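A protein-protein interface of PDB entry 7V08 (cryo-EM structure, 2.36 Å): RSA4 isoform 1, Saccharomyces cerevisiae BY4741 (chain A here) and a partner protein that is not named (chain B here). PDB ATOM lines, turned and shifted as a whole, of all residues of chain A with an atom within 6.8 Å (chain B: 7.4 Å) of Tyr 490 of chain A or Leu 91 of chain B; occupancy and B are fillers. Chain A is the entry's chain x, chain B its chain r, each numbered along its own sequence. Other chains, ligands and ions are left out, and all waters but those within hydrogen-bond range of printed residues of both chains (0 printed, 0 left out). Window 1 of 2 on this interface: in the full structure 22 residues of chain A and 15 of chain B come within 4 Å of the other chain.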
ATOM      1  N   THR A 145      17.409 -27.040  12.552  1.00  0.00           N
ATOM      2  CA  THR A 145      17.123 -25.883  11.717  1.00  0.00           C
ATOM      3  C   THR A 145      18.386 -25.366  11.041  1.00  0.00           C
ATOM      4  O   THR A 145      19.447 -25.254  11.655  1.00  0.00           O
ATOM      5  CB  THR A 145      16.505 -24.753  12.542  1.00  0.00           C
ATOM      6  OG1 THR A 145      17.525 -24.136  13.331  1.00  0.00           O
ATOM      7  CG2 THR A 145      15.420 -25.281  13.464  1.00  0.00           C
ATOM      8  N   ILE A 146      18.250 -25.039   9.764  1.00  0.00           N
ATOM      9  CA  ILE A 146      19.341 -24.485   8.977  1.00  0.00           C
ATOM     10  C   ILE A 146      19.482 -23.005   9.307  1.00  0.00           C
ATOM     11  O   ILE A 146      18.497 -22.260   9.303  1.00  0.00           O
ATOM     12  CB  ILE A 146      19.082 -24.704   7.479  1.00  0.00           C
ATOM     13  CG1 ILE A 146      19.099 -26.198   7.154  1.00  0.00           C
ATOM     14  CG2 ILE A 146      20.078 -23.944   6.643  1.00  0.00           C
ATOM     15  CD1 ILE A 146      18.280 -26.572   5.944  1.00  0.00           C
ATOM     16  N   LEU A 147      20.701 -22.577   9.607  1.00  0.00           N
ATOM     17  CA  LEU A 147      20.946 -21.208  10.039  1.00  0.00           C
ATOM     18  C   LEU A 147      21.606 -20.339   8.984  1.00  0.00           C
ATOM     19  O   LEU A 147      21.271 -19.160   8.873  1.00  0.00           O
ATOM     20  CB  LEU A 147      21.805 -21.202  11.306  1.00  0.00           C
ATOM     21  CG  LEU A 147      21.319 -22.114  12.433  1.00  0.00           C
ATOM     22  CD1 LEU A 147      22.207 -21.982  13.653  1.00  0.00           C
ATOM     23  CD2 LEU A 147      19.876 -21.813  12.786  1.00  0.00           C
ATOM     24  N   CYS A 148      22.543 -20.874   8.206  1.00  0.00           N
ATOM     25  CA  CYS A 148      23.315 -20.022   7.314  1.00  0.00           C
ATOM     26  C   CYS A 148      23.694 -20.789   6.058  1.00  0.00           C
ATOM     27  O   CYS A 148      23.767 -22.018   6.069  1.00  0.00           O
ATOM     28  CB  CYS A 148      24.569 -19.498   8.020  1.00  0.00           C
ATOM     29  SG  CYS A 148      25.446 -20.765   8.949  1.00  0.00           S
ATOM     30  N   ASN A 406      16.177  -5.105   9.377  1.00  0.00           N
ATOM     31  CA  ASN A 406      16.980  -6.271   9.715  1.00  0.00           C
ATOM     32  C   ASN A 406      18.154  -6.455   8.766  1.00  0.00           C
ATOM     33  O   ASN A 406      19.253  -6.801   9.211  1.00  0.00           O
ATOM     34  CB  ASN A 406      16.112  -7.527   9.730  1.00  0.00           C
ATOM     35  CG  ASN A 406      16.876  -8.748  10.194  1.00  0.00           C
ATOM     36  OD1 ASN A 406      17.171  -8.893  11.377  1.00  0.00           O
ATOM     37  ND2 ASN A 406      17.211  -9.631   9.262  1.00  0.00           N
ATOM     38  N   PHE A 422      11.197  -5.610   9.237  1.00  0.00           N
ATOM     39  CA  PHE A 422      10.211  -6.423   9.929  1.00  0.00           C
ATOM     40  C   PHE A 422       8.780  -5.951   9.695  1.00  0.00           C
ATOM     41  O   PHE A 422       7.849  -6.581  10.202  1.00  0.00           O
ATOM     42  CB  PHE A 422      10.491  -6.458  11.437  1.00  0.00           C
ATOM     43  CG  PHE A 422      11.454  -7.532  11.860  1.00  0.00           C
ATOM     44  CD1 PHE A 422      12.437  -7.994  11.000  1.00  0.00           C
ATOM     45  CD2 PHE A 422      11.370  -8.089  13.121  1.00  0.00           C
ATOM     46  CE1 PHE A 422      13.316  -8.977  11.397  1.00  0.00           C
ATOM     47  CE2 PHE A 422      12.245  -9.071  13.521  1.00  0.00           C
ATOM     48  CZ  PHE A 422      13.218  -9.518  12.660  1.00  0.00           C
ATOM     49  N   SER A 446       7.515 -10.805   8.397  1.00  0.00           N
ATOM     50  CA  SER A 446       8.757 -10.040   8.444  1.00  0.00           C
ATOM     51  C   SER A 446       9.800 -10.623   7.501  1.00  0.00           C
ATOM     52  O   SER A 446       9.996 -11.838   7.438  1.00  0.00           O
ATOM     53  CB  SER A 446       9.301  -9.998   9.870  1.00  0.00           C
ATOM     54  OG  SER A 446       9.435 -11.297  10.409  1.00  0.00           O
ATOM     55  N   TYR A 448      13.382 -11.455   6.461  1.00  0.00           N
ATOM     56  CA  TYR A 448      14.618 -11.690   7.195  1.00  0.00           C
ATOM     57  C   TYR A 448      15.848 -11.203   6.439  1.00  0.00           C
ATOM     58  O   TYR A 448      16.586 -10.357   6.950  1.00  0.00           O
ATOM     59  CB  TYR A 448      14.738 -13.169   7.536  1.00  0.00           C
ATOM     60  CG  TYR A 448      13.740 -13.578   8.583  1.00  0.00           C
ATOM     61  CD1 TYR A 448      13.409 -12.712   9.617  1.00  0.00           C
ATOM     62  CD2 TYR A 448      13.113 -14.809   8.533  1.00  0.00           C
ATOM     63  CE1 TYR A 448      12.501 -13.070  10.578  1.00  0.00           C
ATOM     64  CE2 TYR A 448      12.205 -15.176   9.487  1.00  0.00           C
ATOM     65  CZ  TYR A 448      11.899 -14.302  10.508  1.00  0.00           C
ATOM     66  OH  TYR A 448      10.987 -14.667  11.461  1.00  0.00           O
ATOM     67  N   GLN A 449      16.081 -11.699   5.227  1.00  0.00           N
ATOM     68  CA  GLN A 449      17.211 -11.205   4.461  1.00  0.00           C
ATOM     69  C   GLN A 449      16.954 -11.326   2.967  1.00  0.00           C
ATOM     70  O   GLN A 449      15.943 -11.881   2.507  1.00  0.00           O
ATOM     71  CB  GLN A 449      18.514 -11.906   4.853  1.00  0.00           C
ATOM     72  CG  GLN A 449      18.627 -13.357   4.492  1.00  0.00           C
ATOM     73  CD  GLN A 449      19.975 -13.902   4.899  1.00  0.00           C
ATOM     74  OE1 GLN A 449      20.420 -14.938   4.409  1.00  0.00           O
ATOM     75  NE2 GLN A 449      20.640 -13.192   5.800  1.00  0.00           N
ATOM     76  N   CYS A 462      13.871 -13.740   1.353  1.00  0.00           N
ATOM     77  CA  CYS A 462      13.252 -14.821   2.106  1.00  0.00           C
ATOM     78  C   CYS A 462      12.439 -14.229   3.245  1.00  0.00           C
ATOM     79  O   CYS A 462      12.796 -13.176   3.782  1.00  0.00           O
ATOM     80  CB  CYS A 462      14.297 -15.791   2.659  1.00  0.00           C
ATOM     81  SG  CYS A 462      15.426 -15.083   3.874  1.00  0.00           S
ATOM     82  N   SER A 463      11.348 -14.887   3.623  1.00  0.00           N
ATOM     83  CA  SER A 463      10.549 -14.305   4.694  1.00  0.00           C
ATOM     84  C   SER A 463      10.193 -15.325   5.768  1.00  0.00           C
ATOM     85  O   SER A 463      10.413 -16.530   5.634  1.00  0.00           O
ATOM     86  CB  SER A 463       9.272 -13.670   4.144  1.00  0.00           C
ATOM     87  OG  SER A 463       8.508 -13.080   5.174  1.00  0.00           O
ATOM     88  N   LYS A 464       9.642 -14.788   6.856  1.00  0.00           N
ATOM     89  CA  LYS A 464       8.975 -15.543   7.904  1.00  0.00           C
ATOM     90  C   LYS A 464       7.706 -16.232   7.412  1.00  0.00           C
ATOM     91  O   LYS A 464       7.275 -17.207   8.034  1.00  0.00           O
ATOM     92  CB  LYS A 464       8.665 -14.588   9.065  1.00  0.00           C
ATOM     93  CG  LYS A 464       8.023 -15.182  10.303  1.00  0.00           C
ATOM     94  CD  LYS A 464       7.697 -14.091  11.309  1.00  0.00           C
ATOM     95  CE  LYS A 464       7.319 -14.660  12.669  1.00  0.00           C
ATOM     96  NZ  LYS A 464       5.965 -15.282  12.674  1.00  0.00           N
ATOM     97  N   ASP A 487       8.219 -24.295   6.561  1.00  0.00           N
ATOM     98  CA  ASP A 487       8.385 -23.528   7.787  1.00  0.00           C
ATOM     99  C   ASP A 487       9.183 -22.271   7.458  1.00  0.00           C
ATOM    100  O   ASP A 487       9.474 -21.995   6.291  1.00  0.00           O
ATOM    101  CB  ASP A 487       9.051 -24.395   8.861  1.00  0.00           C
ATOM    102  CG  ASP A 487       8.555 -24.081  10.254  1.00  0.00           C
ATOM    103  OD1 ASP A 487       7.924 -23.019  10.440  1.00  0.00           O
ATOM    104  OD2 ASP A 487       8.798 -24.896  11.168  1.00  0.00           O
ATOM    105  N   GLU A 488       9.526 -21.499   8.490  1.00  0.00           N
ATOM    106  CA  GLU A 488      10.184 -20.214   8.287  1.00  0.00           C
ATOM    107  C   GLU A 488      11.529 -20.387   7.595  1.00  0.00           C
ATOM    108  O   GLU A 488      12.267 -21.338   7.862  1.00  0.00           O
ATOM    109  CB  GLU A 488      10.390 -19.494   9.622  1.00  0.00           C
ATOM    110  CG  GLU A 488       9.136 -19.342  10.456  1.00  0.00           C
ATOM    111  CD  GLU A 488       9.332 -18.440  11.658  1.00  0.00           C
ATOM    112  OE1 GLU A 488       9.977 -17.380  11.518  1.00  0.00           O
ATOM    113  OE2 GLU A 488       8.840 -18.794  12.748  1.00  0.00           O
ATOM    114  N   VAL A 489      11.838 -19.460   6.697  1.00  0.00           N
ATOM    115  CA  VAL A 489      13.076 -19.476   5.932  1.00  0.00           C
ATOM    116  C   VAL A 489      14.013 -18.443   6.532  1.00  0.00           C
ATOM    117  O   VAL A 489      13.652 -17.271   6.665  1.00  0.00           O
ATOM    118  CB  VAL A 489      12.826 -19.186   4.446  1.00  0.00           C
ATOM    119  CG1 VAL A 489      14.126 -19.300   3.667  1.00  0.00           C
ATOM    120  CG2 VAL A 489      11.779 -20.132   3.907  1.00  0.00           C
ATOM    121  N   TYR A 490      15.220 -18.872   6.880  1.00  0.00           N
ATOM    122  CA  TYR A 490      16.176 -17.995   7.535  1.00  0.00           C
ATOM    123  C   TYR A 490      17.242 -17.458   6.594  1.00  0.00           C
ATOM    124  O   TYR A 490      17.618 -16.290   6.708  1.00  0.00           O
ATOM    125  CB  TYR A 490      16.843 -18.725   8.701  1.00  0.00           C
ATOM    126  CG  TYR A 490      15.915 -19.003   9.859  1.00  0.00           C
ATOM    127  CD1 TYR A 490      14.854 -18.154  10.145  1.00  0.00           C
ATOM    128  CD2 TYR A 490      16.100 -20.108  10.667  1.00  0.00           C
ATOM    129  CE1 TYR A 490      14.004 -18.404  11.201  1.00  0.00           C
ATOM    130  CE2 TYR A 490      15.254 -20.365  11.727  1.00  0.00           C
ATOM    131  CZ  TYR A 490      14.209 -19.510  11.986  1.00  0.00           C
ATOM    132  OH  TYR A 490      13.370 -19.765  13.044  1.00  0.00           O
ATOM    133  N   THR A 491      17.740 -18.260   5.662  1.00  0.00           N
ATOM    134  CA  THR A 491      18.866 -17.835   4.846  1.00  0.00           C
ATOM    135  C   THR A 491      18.572 -18.061   3.370  1.00  0.00           C
ATOM    136  O   THR A 491      17.890 -19.022   2.999  1.00  0.00           O
ATOM    137  CB  THR A 491      20.164 -18.567   5.264  1.00  0.00           C
ATOM    138  OG1 THR A 491      21.259 -18.113   4.457  1.00  0.00           O
ATOM    139  CG2 THR A 491      20.022 -20.077   5.126  1.00  0.00           C
ATOM    140  N   VAL A 492      19.092 -17.158   2.536  1.00  0.00           N
ATOM    141  CA  VAL A 492      18.935 -17.228   1.088  1.00  0.00           C
ATOM    142  C   VAL A 492      20.206 -16.696   0.439  1.00  0.00           C
ATOM    143  O   VAL A 492      20.879 -15.814   0.980  1.00  0.00           O
ATOM    144  CB  VAL A 492      17.678 -16.453   0.610  1.00  0.00           C
ATOM    145  CG1 VAL A 492      17.877 -14.952   0.710  1.00  0.00           C
ATOM    146  CG2 VAL A 492      17.296 -16.851  -0.802  1.00  0.00           C
ATOM    147  N   SER A 503      18.165 -21.764  -0.445  1.00  0.00           N
ATOM    148  CA  SER A 503      17.438 -21.247   0.706  1.00  0.00           C
ATOM    149  C   SER A 503      17.335 -22.324   1.777  1.00  0.00           C
ATOM    150  O   SER A 503      17.414 -23.522   1.487  1.00  0.00           O
ATOM    151  CB  SER A 503      16.037 -20.762   0.320  1.00  0.00           C
ATOM    152  OG  SER A 503      15.186 -21.858   0.060  1.00  0.00           O
ATOM    153  N   GLY A 504      17.155 -21.884   3.019  1.00  0.00           N
ATOM    154  CA  GLY A 504      17.023 -22.817   4.123  1.00  0.00           C
ATOM    155  C   GLY A 504      16.426 -22.172   5.350  1.00  0.00           C
ATOM    156  O   GLY A 504      16.564 -20.963   5.570  1.00  0.00           O
ATOM    157  N   GLY A 505      15.776 -22.995   6.173  1.00  0.00           N
ATOM    158  CA  GLY A 505      15.201 -22.528   7.422  1.00  0.00           C
ATOM    159  C   GLY A 505      14.780 -23.627   8.379  1.00  0.00           C
ATOM    160  O   GLY A 505      15.485 -24.627   8.537  1.00  0.00           O
ATOM    161  N   LYS A 506      13.622 -23.460   9.017  1.00  0.00           N
ATOM    162  CA  LYS A 506      13.166 -24.369  10.062  1.00  0.00           C
ATOM    163  C   LYS A 506      12.710 -25.727   9.550  1.00  0.00           C
ATOM    164  O   LYS A 506      12.485 -26.623  10.370  1.00  0.00           O
ATOM    165  CB  LYS A 506      12.009 -23.748  10.846  1.00  0.00           C
ATOM    166  CG  LYS A 506      12.345 -22.487  11.594  1.00  0.00           C
ATOM    167  CD  LYS A 506      11.184 -22.075  12.484  1.00  0.00           C
ATOM    168  CE  LYS A 506      10.924 -23.116  13.559  1.00  0.00           C
ATOM    169  NZ  LYS A 506       9.687 -22.825  14.323  1.00  0.00           N
ATOM    170  N   ASP B  85      16.068 -23.602  20.594  1.00  0.00           N
ATOM    171  CA  ASP B  85      15.227 -23.432  19.415  1.00  0.00           C
ATOM    172  C   ASP B  85      16.070 -23.429  18.142  1.00  0.00           C
ATOM    173  O   ASP B  85      15.558 -23.719  17.059  1.00  0.00           O
ATOM    174  CB  ASP B  85      14.414 -22.137  19.517  1.00  0.00           C
ATOM    175  CG  ASP B  85      13.357 -22.022  18.432  1.00  0.00           C
ATOM    176  OD1 ASP B  85      12.489 -22.914  18.350  1.00  0.00           O
ATOM    177  OD2 ASP B  85      13.385 -21.037  17.670  1.00  0.00           O
ATOM    178  N   ALA B  86      17.361 -23.114  18.294  1.00  0.00           N
ATOM    179  CA  ALA B  86      18.317 -22.992  17.190  1.00  0.00           C
ATOM    180  C   ALA B  86      17.863 -21.925  16.188  1.00  0.00           C
ATOM    181  O   ALA B  86      17.409 -22.213  15.083  1.00  0.00           O
ATOM    182  CB  ALA B  86      18.557 -24.345  16.509  1.00  0.00           C
ATOM    183  N   LEU B  87      17.973 -20.657  16.642  1.00  0.00           N
ATOM    184  CA  LEU B  87      17.722 -19.371  16.004  1.00  0.00           C
ATOM    185  C   LEU B  87      18.950 -18.887  15.233  1.00  0.00           C
ATOM    186  O   LEU B  87      20.079 -19.268  15.554  1.00  0.00           O
ATOM    187  CB  LEU B  87      17.341 -18.330  17.054  1.00  0.00           C
ATOM    188  CG  LEU B  87      16.002 -18.501  17.768  1.00  0.00           C
ATOM    189  CD1 LEU B  87      15.913 -17.565  18.958  1.00  0.00           C
ATOM    190  CD2 LEU B  87      14.862 -18.241  16.807  1.00  0.00           C
ATOM    191  N   PRO B  88      18.771 -18.032  14.205  1.00  0.00           N
ATOM    192  CA  PRO B  88      19.934 -17.438  13.528  1.00  0.00           C
ATOM    193  C   PRO B  88      20.545 -16.302  14.334  1.00  0.00           C
ATOM    194  O   PRO B  88      20.070 -16.003  15.432  1.00  0.00           O
ATOM    195  CB  PRO B  88      19.357 -16.927  12.202  1.00  0.00           C
ATOM    196  CG  PRO B  88      17.944 -17.394  12.157  1.00  0.00           C
ATOM    197  CD  PRO B  88      17.514 -17.642  13.550  1.00  0.00           C
ATOM    198  N   THR B  89      21.578 -15.651  13.793  1.00  0.00           N
ATOM    199  CA  THR B  89      22.266 -14.594  14.533  1.00  0.00           C
ATOM    200  C   THR B  89      21.372 -13.380  14.752  1.00  0.00           C
ATOM    201  O   THR B  89      21.475 -12.709  15.783  1.00  0.00           O
ATOM    202  CB  THR B  89      23.544 -14.170  13.806  1.00  0.00           C
ATOM    203  OG1 THR B  89      23.212 -13.679  12.503  1.00  0.00           O
ATOM    204  CG2 THR B  89      24.497 -15.337  13.673  1.00  0.00           C
ATOM    205  N   TYR B  90      20.504 -13.067  13.795  1.00  0.00           N
ATOM    206  CA  TYR B  90      19.658 -11.885  13.920  1.00  0.00           C
ATOM    207  C   TYR B  90      18.377 -12.137  14.705  1.00  0.00           C
ATOM    208  O   TYR B  90      17.587 -11.206  14.871  1.00  0.00           O
ATOM    209  CB  TYR B  90      19.310 -11.323  12.536  1.00  0.00           C
ATOM    210  CG  TYR B  90      18.791 -12.353  11.562  1.00  0.00           C
ATOM    211  CD1 TYR B  90      17.440 -12.680  11.522  1.00  0.00           C
ATOM    212  CD2 TYR B  90      19.648 -12.997  10.680  1.00  0.00           C
ATOM    213  CE1 TYR B  90      16.963 -13.623  10.637  1.00  0.00           C
ATOM    214  CE2 TYR B  90      19.178 -13.940   9.791  1.00  0.00           C
ATOM    215  CZ  TYR B  90      17.836 -14.246   9.774  1.00  0.00           C
ATOM    216  OH  TYR B  90      17.360 -15.182   8.894  1.00  0.00           O
ATOM    217  N   LEU B  91      18.137 -13.357  15.181  1.00  0.00           N
ATOM    218  CA  LEU B  91      16.977 -13.601  16.026  1.00  0.00           C
ATOM    219  C   LEU B  91      17.335 -13.916  17.474  1.00  0.00           C
ATOM    220  O   LEU B  91      16.450 -13.861  18.336  1.00  0.00           O
ATOM    221  CB  LEU B  91      16.118 -14.733  15.446  1.00  0.00           C
ATOM    222  CG  LEU B  91      15.432 -14.421  14.107  1.00  0.00           C
ATOM    223  CD1 LEU B  91      14.474 -15.521  13.701  1.00  0.00           C
ATOM    224  CD2 LEU B  91      14.711 -13.081  14.144  1.00  0.00           C
ATOM    225  N   LEU B  92      18.584 -14.254  17.768  1.00  0.00           N
ATOM    226  CA  LEU B  92      18.983 -14.342  19.162  1.00  0.00           C
ATOM    227  C   LEU B  92      19.258 -12.943  19.712  1.00  0.00           C
ATOM    228  O   LEU B  92      19.464 -11.985  18.963  1.00  0.00           O
ATOM    229  CB  LEU B  92      20.196 -15.261  19.330  1.00  0.00           C
ATOM    230  CG  LEU B  92      20.081 -16.753  19.015  1.00  0.00           C
ATOM    231  CD1 LEU B  92      21.428 -17.446  19.108  1.00  0.00           C
ATOM    232  CD2 LEU B  92      19.074 -17.412  19.936  1.00  0.00           C
ATOM    233  N   ASP B  93      19.267 -12.843  21.045  1.00  0.00           N
ATOM    234  CA  ASP B  93      19.190 -11.584  21.798  1.00  0.00           C
ATOM    235  C   ASP B  93      17.876 -10.853  21.553  1.00  0.00           C
ATOM    236  O   ASP B  93      17.780  -9.646  21.789  1.00  0.00           O
ATOM    237  CB  ASP B  93      20.362 -10.643  21.502  1.00  0.00           C
ATOM    238  CG  ASP B  93      21.657 -11.135  22.080  1.00  0.00           C
ATOM    239  OD1 ASP B  93      21.611 -12.038  22.942  1.00  0.00           O
ATOM    240  OD2 ASP B  93      22.721 -10.633  21.663  1.00  0.00           O
ATOM    241  N   ARG B  94      16.863 -11.568  21.074  1.00  0.00           N
ATOM    242  CA  ARG B  94      15.530 -11.026  20.880  1.00  0.00           C
ATOM    243  C   ARG B  94      14.522 -11.965  21.522  1.00  0.00           C
ATOM    244  O   ARG B  94      14.714 -13.185  21.528  1.00  0.00           O
ATOM    245  CB  ARG B  94      15.205 -10.840  19.399  1.00  0.00           C
ATOM    246  CG  ARG B  94      16.150  -9.907  18.660  1.00  0.00           C
ATOM    247  CD  ARG B  94      15.674  -9.682  17.242  1.00  0.00           C
ATOM    248  NE  ARG B  94      16.544  -8.779  16.501  1.00  0.00           N
ATOM    249  CZ  ARG B  94      16.482  -7.457  16.560  1.00  0.00           C
ATOM    250  NH1 ARG B  94      15.617  -6.841  17.345  1.00  0.00           N
ATOM    251  NH2 ARG B  94      17.317  -6.737  15.820  1.00  0.00           N
ATOM    252  N   GLU B  95      13.461 -11.395  22.067  1.00  0.00           N
ATOM    253  CA  GLU B  95      12.391 -12.155  22.687  1.00  0.00           C
ATOM    254  C   GLU B  95      11.161 -12.104  21.784  1.00  0.00           C
ATOM    255  O   GLU B  95      11.173 -11.467  20.725  1.00  0.00           O
ATOM    256  CB  GLU B  95      12.118 -11.608  24.089  1.00  0.00           C
ATOM    257  CG  GLU B  95      13.394 -11.270  24.857  1.00  0.00           C
ATOM    258  CD  GLU B  95      13.163 -11.105  26.346  1.00  0.00           C
ATOM    259  OE1 GLU B  95      11.995 -10.945  26.753  1.00  0.00           O
ATOM    260  OE2 GLU B  95      14.153 -11.149  27.109  1.00  0.00           O
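The side-chain hydroxyl (OG1) of Thr 145 of chain A is in hydrogen-bond range of the backbone carbonyl oxygen (O) of Ala 86 of chain B, 2.6 Å away.
OH of Tyr 90 of chain B is in hydrogen-bond range of O of Tyr 490 of chain A, 2.5 Å away.
The backbone carbonyl oxygen (O) of Tyr 90 of chain B is in hydrogen-bond range of the guanidinium group (NE) of Arg 94 of chain B (3.1 Å).
The side-chain amide nitrogen (ND2) of Asn 406 of chain A is in hydrogen-bond range of the backbone carbonyl oxygen (O) of Tyr 448 of chain A, 2.5 Å away.
The backbone NH (N) of Tyr 448 of chain A lies within hydrogen-bond range of the backbone carbonyl oxygen (O) of Cys 462 of chain A (3.2 Å).
The side-chain hydroxyl (OH) of Tyr 448 of chain A is in hydrogen-bond range of the side-chain carboxylate (OE1) of Glu 488 of chain A, at 2.9 Å.
SG of Cys 462 of chain A lies within hydrogen-bond range of O of Tyr 490 of chain A.
The backbone carbonyl oxygen (O) of Gly 504 of chain A lies within hydrogen-bond range of the backbone NH (N) of Tyr 490 of chain A, 2.8 Å away.
Thr 145 of chain A touches Asp 85 of chain B (CG2 to O, 3.9 Å).
Leu 147 of chain A touches Ala 86 of chain B.
Leu 87 of chain B touches Leu 147 of chain A (O to CD2, 3.8 Å).
OD1 of Asn 406 of chain A touches CB of Tyr 90 of chain B, 3.4 Å away.
OH of Tyr 90 of chain B touches CB of Tyr 448 of chain A (3.6 Å).
Pro 88 of chain B touches Tyr 490 of chain A.
Leu 91 of chain B touches Tyr 490 of chain A.
Of the printed residues of chain B, Tyr 490 of chain A touches Pro 88 (3.5 Å), Tyr 90 (2.5 Å) and Leu 91 (3.8 Å).
Of chain A, only Tyr 490 comes within 4 Å of Leu 91 of chain B.
Of the printed residues of chain B, Thr 145 of chain A touches Asp 85 and Ala 86.
Printed residues of chain B within 4 Å of Asn 406 of chain A: Tyr 90.
Printed residues of chain A within 4 Å of Leu 87 of chain B: Leu 147 (3.8 Å).
Gln 449 of chain A touches none of the printed residues of chain B.
The nearest residue of chain B that does not touch Tyr 490 of chain A is Leu 87 of chain B (4.3 Å).
The nearest residue of chain A that does not touch Leu 91 of chain B is Phe 422 of chain A (4.1 Å).
Hydrophobic or aromatic side chains of chain B within 4 Å of the printed part of chain A: Ala 86, Pro 88, Tyr 90 and Leu 91.
Of the 22 printed residues of chain A, 5 touch a printed residue of chain B.
Printed residues of chain A that touch a printed residue of chain B: Thr 145, Leu 147, Asn 406, Tyr 448 and Tyr 490.
Hydrophobic or aromatic side chains of chain A that line the printed part of chain B: Leu 147, Tyr 448 and Tyr 490.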
